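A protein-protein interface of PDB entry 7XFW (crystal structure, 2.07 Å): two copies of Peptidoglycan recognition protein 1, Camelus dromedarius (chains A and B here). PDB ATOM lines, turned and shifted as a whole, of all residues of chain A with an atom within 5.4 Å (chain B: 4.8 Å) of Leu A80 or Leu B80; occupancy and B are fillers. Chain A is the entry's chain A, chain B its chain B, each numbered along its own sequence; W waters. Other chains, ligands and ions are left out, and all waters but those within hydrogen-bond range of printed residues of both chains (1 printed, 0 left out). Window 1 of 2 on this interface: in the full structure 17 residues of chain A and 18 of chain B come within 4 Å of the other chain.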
ATOM      1  N   VAL A  10      27.618  27.590  31.174  1.00  0.00           N
ATOM      2  CA  VAL A  10      28.283  28.861  31.555  1.00  0.00           C
ATOM      3  C   VAL A  10      27.723  29.196  32.931  1.00  0.00           C
ATOM      4  O   VAL A  10      26.510  29.392  33.062  1.00  0.00           O
ATOM      5  CB  VAL A  10      28.041  29.972  30.515  1.00  0.00           C
ATOM      6  CG1 VAL A  10      28.617  31.311  30.944  1.00  0.00           C
ATOM      7  CG2 VAL A  10      28.582  29.583  29.148  1.00  0.00           C
ATOM      8  N   PRO A  46      30.316  33.710  22.438  1.00  0.00           N
ATOM      9  CA  PRO A  46      30.299  33.659  23.897  1.00  0.00           C
ATOM     10  C   PRO A  46      30.236  35.067  24.483  1.00  0.00           C
ATOM     11  O   PRO A  46      29.504  35.272  25.416  1.00  0.00           O
ATOM     12  CB  PRO A  46      31.624  32.964  24.252  1.00  0.00           C
ATOM     13  CG  PRO A  46      31.918  32.129  23.038  1.00  0.00           C
ATOM     14  CD  PRO A  46      31.449  32.960  21.864  1.00  0.00           C
ATOM     15  N   LEU A  74      19.225  29.463  30.045  1.00  0.00           N
ATOM     16  CA  LEU A  74      19.083  30.093  28.705  1.00  0.00           C
ATOM     17  C   LEU A  74      19.974  29.373  27.694  1.00  0.00           C
ATOM     18  O   LEU A  74      21.034  28.838  28.090  1.00  0.00           O
ATOM     19  CB  LEU A  74      19.443  31.571  28.781  1.00  0.00           C
ATOM     20  CG  LEU A  74      18.591  32.370  29.754  1.00  0.00           C
ATOM     21  CD1 LEU A  74      19.188  32.315  31.159  1.00  0.00           C
ATOM     22  CD2 LEU A  74      18.444  33.793  29.281  1.00  0.00           C
ATOM     23  N   ILE A  75      19.519  29.321  26.444  1.00  0.00           N
ATOM     24  CA  ILE A  75      20.290  28.744  25.304  1.00  0.00           C
ATOM     25  C   ILE A  75      20.690  29.883  24.381  1.00  0.00           C
ATOM     26  O   ILE A  75      19.809  30.653  23.972  1.00  0.00           O
ATOM     27  CB  ILE A  75      19.494  27.677  24.547  1.00  0.00           C
ATOM     28  CG1 ILE A  75      18.675  26.787  25.492  1.00  0.00           C
ATOM     29  CG2 ILE A  75      20.433  26.888  23.653  1.00  0.00           C
ATOM     30  CD1 ILE A  75      19.498  25.907  26.415  1.00  0.00           C
ATOM     31  N   GLY A  76      21.992  29.988  24.111  1.00  0.00           N
ATOM     32  CA  GLY A  76      22.556  30.939  23.144  1.00  0.00           C
ATOM     33  C   GLY A  76      22.743  30.276  21.797  1.00  0.00           C
ATOM     34  O   GLY A  76      22.935  29.054  21.747  1.00  0.00           O
ATOM     35  N   ASP A  78      25.319  30.779  20.281  1.00  0.00           N
ATOM     36  CA  ASP A  78      26.764  30.442  20.433  1.00  0.00           C
ATOM     37  C   ASP A  78      26.917  28.952  20.731  1.00  0.00           C
ATOM     38  O   ASP A  78      28.039  28.446  20.628  1.00  0.00           O
ATOM     39  CB  ASP A  78      27.427  31.275  21.522  1.00  0.00           C
ATOM     40  CG  ASP A  78      26.863  31.035  22.910  1.00  0.00           C
ATOM     41  OD1 ASP A  78      25.881  30.251  23.014  1.00  0.00           O
ATOM     42  OD2 ASP A  78      27.417  31.634  23.869  1.00  0.00           O
ATOM     43  N   GLY A  79      25.826  28.276  21.082  1.00  0.00           N
ATOM     44  CA  GLY A  79      25.811  26.825  21.329  1.00  0.00           C
ATOM     45  C   GLY A  79      26.112  26.498  22.778  1.00  0.00           C
ATOM     46  O   GLY A  79      26.306  25.335  23.060  1.00  0.00           O
ATOM     47  N   LEU A  80      26.109  27.492  23.664  1.00  0.00           N
ATOM     48  CA  LEU A  80      26.350  27.316  25.122  1.00  0.00           C
ATOM     49  C   LEU A  80      25.039  27.490  25.896  1.00  0.00           C
ATOM     50  O   LEU A  80      24.146  28.247  25.430  1.00  0.00           O
ATOM     51  CB  LEU A  80      27.400  28.327  25.583  1.00  0.00           C
ATOM     52  CG  LEU A  80      28.734  28.249  24.836  1.00  0.00           C
ATOM     53  CD1 LEU A  80      29.730  29.231  25.430  1.00  0.00           C
ATOM     54  CD2 LEU A  80      29.294  26.843  24.878  1.00  0.00           C
ATOM     55  N   VAL A  81      24.930  26.762  27.003  1.00  0.00           N
ATOM     56  CA  VAL A  81      23.824  26.851  27.993  1.00  0.00           C
ATOM     57  C   VAL A  81      24.254  27.849  29.065  1.00  0.00           C
ATOM     58  O   VAL A  81      25.402  27.757  29.516  1.00  0.00           O
ATOM     59  CB  VAL A  81      23.496  25.472  28.588  1.00  0.00           C
ATOM     60  CG1 VAL A  81      22.333  25.541  29.559  1.00  0.00           C
ATOM     61  CG2 VAL A  81      23.211  24.453  27.498  1.00  0.00           C
ATOM     62  N   TYR A  82      23.394  28.821  29.383  1.00  0.00           N
ATOM     63  CA  TYR A  82      23.679  29.864  30.395  1.00  0.00           C
ATOM     64  C   TYR A  82      22.861  29.545  31.632  1.00  0.00           C
ATOM     65  O   TYR A  82      21.644  29.333  31.545  1.00  0.00           O
ATOM     66  CB  TYR A  82      23.466  31.274  29.858  1.00  0.00           C
ATOM     67  CG  TYR A  82      24.513  31.630  28.842  1.00  0.00           C
ATOM     68  CD1 TYR A  82      24.420  31.154  27.545  1.00  0.00           C
ATOM     69  CD2 TYR A  82      25.638  32.357  29.195  1.00  0.00           C
ATOM     70  CE1 TYR A  82      25.389  31.447  26.602  1.00  0.00           C
ATOM     71  CE2 TYR A  82      26.608  32.677  28.258  1.00  0.00           C
ATOM     72  CZ  TYR A  82      26.496  32.200  26.963  1.00  0.00           C
ATOM     73  OH  TYR A  82      27.451  32.489  26.033  1.00  0.00           O
ATOM     74  N   ARG A 119      23.328  24.022  16.860  1.00  0.00           N
ATOM     75  CA  ARG A 119      24.186  23.919  18.073  1.00  0.00           C
ATOM     76  C   ARG A 119      23.391  24.416  19.287  1.00  0.00           C
ATOM     77  O   ARG A 119      23.593  23.891  20.378  1.00  0.00           O
ATOM     78  CB  ARG A 119      25.505  24.661  17.877  1.00  0.00           C
ATOM     79  CG  ARG A 119      25.379  26.168  17.792  1.00  0.00           C
ATOM     80  CD  ARG A 119      26.725  26.797  17.491  1.00  0.00           C
ATOM     81  NE  ARG A 119      26.467  28.109  16.949  1.00  0.00           N
ATOM     82  CZ  ARG A 119      26.268  28.361  15.674  1.00  0.00           C
ATOM     83  NH1 ARG A 119      26.357  27.382  14.793  1.00  0.00           N
ATOM     84  NH2 ARG A 119      25.989  29.594  15.288  1.00  0.00           N
ATOM     85  N   ALA A 123      22.637  21.936  22.392  1.00  0.00           N
ATOM     86  CA  ALA A 123      22.863  22.453  23.765  1.00  0.00           C
ATOM     87  C   ALA A 123      21.624  22.171  24.625  1.00  0.00           C
ATOM     88  O   ALA A 123      21.769  21.628  25.733  1.00  0.00           O
ATOM     89  CB  ALA A 123      23.202  23.921  23.716  1.00  0.00           C
ATOM     90  N   VAL B  10      29.910  19.464  17.726  1.00  0.00           N
ATOM     91  CA  VAL B  10      29.727  19.916  16.318  1.00  0.00           C
ATOM     92  C   VAL B  10      30.070  18.729  15.418  1.00  0.00           C
ATOM     93  O   VAL B  10      31.181  18.189  15.477  1.00  0.00           O
ATOM     94  CB  VAL B  10      30.581  21.153  16.012  1.00  0.00           C
ATOM     95  CG1 VAL B  10      30.285  21.679  14.617  1.00  0.00           C
ATOM     96  CG2 VAL B  10      30.392  22.257  17.053  1.00  0.00           C
ATOM     97  N   PRO B  46      31.785  30.264  16.923  1.00  0.00           N
ATOM     98  CA  PRO B  46      31.456  29.072  16.149  1.00  0.00           C
ATOM     99  C   PRO B  46      31.911  29.169  14.683  1.00  0.00           C
ATOM    100  O   PRO B  46      32.468  28.210  14.188  1.00  0.00           O
ATOM    101  CB  PRO B  46      29.928  29.005  16.264  1.00  0.00           C
ATOM    102  CG  PRO B  46      29.647  29.629  17.617  1.00  0.00           C
ATOM    103  CD  PRO B  46      30.654  30.752  17.729  1.00  0.00           C
ATOM    104  N   LEU B  74      38.531  18.081  18.542  1.00  0.00           N
ATOM    105  CA  LEU B  74      39.183  19.410  18.655  1.00  0.00           C
ATOM    106  C   LEU B  74      38.366  20.299  19.606  1.00  0.00           C
ATOM    107  O   LEU B  74      37.134  20.126  19.711  1.00  0.00           O
ATOM    108  CB  LEU B  74      39.321  20.033  17.263  1.00  0.00           C
ATOM    109  CG  LEU B  74      40.275  19.316  16.297  1.00  0.00           C
ATOM    110  CD1 LEU B  74      39.584  18.184  15.549  1.00  0.00           C
ATOM    111  CD2 LEU B  74      40.883  20.288  15.287  1.00  0.00           C
ATOM    112  N   ILE B  75      39.032  21.222  20.292  1.00  0.00           N
ATOM    113  CA  ILE B  75      38.367  22.160  21.241  1.00  0.00           C
ATOM    114  C   ILE B  75      38.632  23.590  20.797  1.00  0.00           C
ATOM    115  O   ILE B  75      39.813  23.951  20.644  1.00  0.00           O
ATOM    116  CB  ILE B  75      38.864  21.930  22.666  1.00  0.00           C
ATOM    117  CG1 ILE B  75      38.919  20.443  22.992  1.00  0.00           C
ATOM    118  CG2 ILE B  75      38.005  22.715  23.651  1.00  0.00           C
ATOM    119  CD1 ILE B  75      37.568  19.802  23.048  1.00  0.00           C
ATOM    120  N   GLY B  76      37.572  24.378  20.621  1.00  0.00           N
ATOM    121  CA  GLY B  76      37.685  25.804  20.245  1.00  0.00           C
ATOM    122  C   GLY B  76      37.619  26.706  21.459  1.00  0.00           C
ATOM    123  O   GLY B  76      37.028  26.305  22.484  1.00  0.00           O
ATOM    124  N   ASP B  78      35.658  28.896  21.488  1.00  0.00           N
ATOM    125  CA  ASP B  78      34.187  29.133  21.429  1.00  0.00           C
ATOM    126  C   ASP B  78      33.494  28.272  22.496  1.00  0.00           C
ATOM    127  O   ASP B  78      32.297  28.510  22.756  1.00  0.00           O
ATOM    128  CB  ASP B  78      33.632  28.867  20.024  1.00  0.00           C
ATOM    129  CG  ASP B  78      33.756  27.430  19.539  1.00  0.00           C
ATOM    130  OD1 ASP B  78      34.321  26.612  20.278  1.00  0.00           O
ATOM    131  OD2 ASP B  78      33.251  27.127  18.426  1.00  0.00           O
ATOM    132  N   GLY B  79      34.204  27.293  23.069  1.00  0.00           N
ATOM    133  CA  GLY B  79      33.687  26.407  24.127  1.00  0.00           C
ATOM    134  C   GLY B  79      32.885  25.239  23.576  1.00  0.00           C
ATOM    135  O   GLY B  79      32.148  24.621  24.356  1.00  0.00           O
ATOM    136  N   LEU B  80      33.036  24.944  22.282  1.00  0.00           N
ATOM    137  CA  LEU B  80      32.445  23.757  21.595  1.00  0.00           C
ATOM    138  C   LEU B  80      33.527  22.737  21.259  1.00  0.00           C
ATOM    139  O   LEU B  80      34.656  23.140  20.916  1.00  0.00           O
ATOM    140  CB  LEU B  80      31.759  24.198  20.298  1.00  0.00           C
ATOM    141  CG  LEU B  80      30.750  25.337  20.432  1.00  0.00           C
ATOM    142  CD1 LEU B  80      30.076  25.584  19.093  1.00  0.00           C
ATOM    143  CD2 LEU B  80      29.732  25.031  21.511  1.00  0.00           C
ATOM    144  N   VAL B  81      33.141  21.469  21.300  1.00  0.00           N
ATOM    145  CA  VAL B  81      33.942  20.328  20.802  1.00  0.00           C
ATOM    146  C   VAL B  81      33.593  20.110  19.334  1.00  0.00           C
ATOM    147  O   VAL B  81      32.396  20.233  18.993  1.00  0.00           O
ATOM    148  CB  VAL B  81      33.687  19.083  21.652  1.00  0.00           C
ATOM    149  CG1 VAL B  81      34.588  17.954  21.246  1.00  0.00           C
ATOM    150  CG2 VAL B  81      33.855  19.392  23.127  1.00  0.00           C
ATOM    151  N   TYR B  82      34.629  19.888  18.511  1.00  0.00           N
ATOM    152  CA  TYR B  82      34.564  19.615  17.049  1.00  0.00           C
ATOM    153  C   TYR B  82      34.941  18.157  16.807  1.00  0.00           C
ATOM    154  O   TYR B  82      35.996  17.706  17.223  1.00  0.00           O
ATOM    155  CB  TYR B  82      35.464  20.589  16.291  1.00  0.00           C
ATOM    156  CG  TYR B  82      34.926  21.983  16.338  1.00  0.00           C
ATOM    157  CD1 TYR B  82      35.174  22.810  17.416  1.00  0.00           C
ATOM    158  CD2 TYR B  82      34.056  22.425  15.358  1.00  0.00           C
ATOM    159  CE1 TYR B  82      34.609  24.072  17.494  1.00  0.00           C
ATOM    160  CE2 TYR B  82      33.490  23.683  15.418  1.00  0.00           C
ATOM    161  CZ  TYR B  82      33.771  24.514  16.482  1.00  0.00           C
ATOM    162  OH  TYR B  82      33.202  25.750  16.513  1.00  0.00           O
ATOM    163  N   ARG B 119      35.557  27.993  29.320  1.00  0.00           N
ATOM    164  CA  ARG B 119      34.521  27.280  28.504  1.00  0.00           C
ATOM    165  C   ARG B 119      35.188  26.206  27.637  1.00  0.00           C
ATOM    166  O   ARG B 119      34.617  25.121  27.518  1.00  0.00           O
ATOM    167  CB  ARG B 119      33.674  28.231  27.652  1.00  0.00           C
ATOM    168  CG  ARG B 119      34.401  28.879  26.485  1.00  0.00           C
ATOM    169  CD  ARG B 119      33.532  29.929  25.817  1.00  0.00           C
ATOM    170  NE  ARG B 119      34.403  30.936  25.253  1.00  0.00           N
ATOM    171  CZ  ARG B 119      34.890  31.973  25.911  1.00  0.00           C
ATOM    172  NH1 ARG B 119      34.528  32.197  27.161  1.00  0.00           N
ATOM    173  NH2 ARG B 119      35.731  32.794  25.308  1.00  0.00           N
ATOM    174  N   ALA B 123      34.345  22.209  28.079  1.00  0.00           N
ATOM    175  CA  ALA B 123      33.963  21.406  26.892  1.00  0.00           C
ATOM    176  C   ALA B 123      34.762  20.094  26.895  1.00  0.00           C
ATOM    177  O   ALA B 123      34.154  19.014  26.701  1.00  0.00           O
ATOM    178  CB  ALA B 123      34.205  22.220  25.647  1.00  0.00           C
HETATM  179  O   HOH W   1      30.345  29.640  21.188  1.00  0.00           O
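Water W1 lies within hydrogen-bond range of O of Asp A78 (2.7 Å) and O of Asp B78 (2.7 Å).
Pro A46 touches Asp B78 (CG to O, 3.6 Å). O of Asp A78 touches CG of Pro B46 (3.6 Å). Asp A78 touches Leu B80 (O to CD1, 3.8 Å). Gly A79 touches Leu B80. CD1 of Leu A80 touches O of Asp B78 (3.8 Å). Leu A80 touches Gly B79. CD2 of Leu A80 touches CD2 of Leu B80, 3.8 Å away. Leu A80 touches Arg B119. Arg A119 touches Pro B46 (NE to CG, 3.6 Å). CD of Arg A119 touches CD1 of Leu B80, at 3.9 Å.
Leu A80 touches just these residues of chain B: Asp B78 (3.8 Å), Gly B79 (3.7 Å), Leu B80 (3.8 Å) and Arg B119 (3.9 Å). Of chain A, only Asp A78, Gly A79, Leu A80 and Arg A119 come within 4 Å of Leu B80. Of the printed residues of chain B, Asp A78 touches Pro B46 and Leu B80. Of the printed residues of chain A, Pro B46 touches Asp A78 (3.6 Å) and Arg A119 (3.6 Å). Of the printed residues of chain A, Gly B79 touches Leu A80 (3.7 Å). The nearest printed residue of chain B that does not touch Leu A80 is Ala B123 (6.8 Å).
Of the 12 printed residues of chain A, 5 touch a printed residue of chain B. Printed residues of chain A that touch a printed residue of chain B: Pro A46, Asp A78, Gly A79, Leu A80 and Arg A119. Hydrophobic or aromatic side chains of chain A that line the printed part of chain B: Pro A46 and Leu A80. Among the printed residues, no Asp or Glu carboxylate lies within 4 Å of a Lys or Arg side-chain nitrogen of the other chain.
The backbone NH (N) of Leu A80 sits at hydrogen-bond distance from the side-chain carboxylate (OD1) of Asp A78 (2.8 Å). The backbone carbonyl oxygen (O) of Pro B46 sits at hydrogen-bond distance from the side-chain hydroxyl (OH) of Tyr B82 (3.5 Å). The side-chain carboxylate of Asp B78 sits at hydrogen-bond distance from the backbone NH of Leu B80 (2.9 Å).
Pro A46 touches Arg B119, and with the chains exchanged Arg A119 touches Pro B46. Asp A78 touches Leu B80, and with the chains exchanged Leu A80 touches Asp B78. Leu A80 touches its own counterpart, Leu B80. Leu A80 touches Arg B119, and with the chains exchanged Arg A119 touches Leu B80. Positions printed for both chains: 10, 46, 74, 75, 76, 78, 79, 80, 81, 82, 119 and 123.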
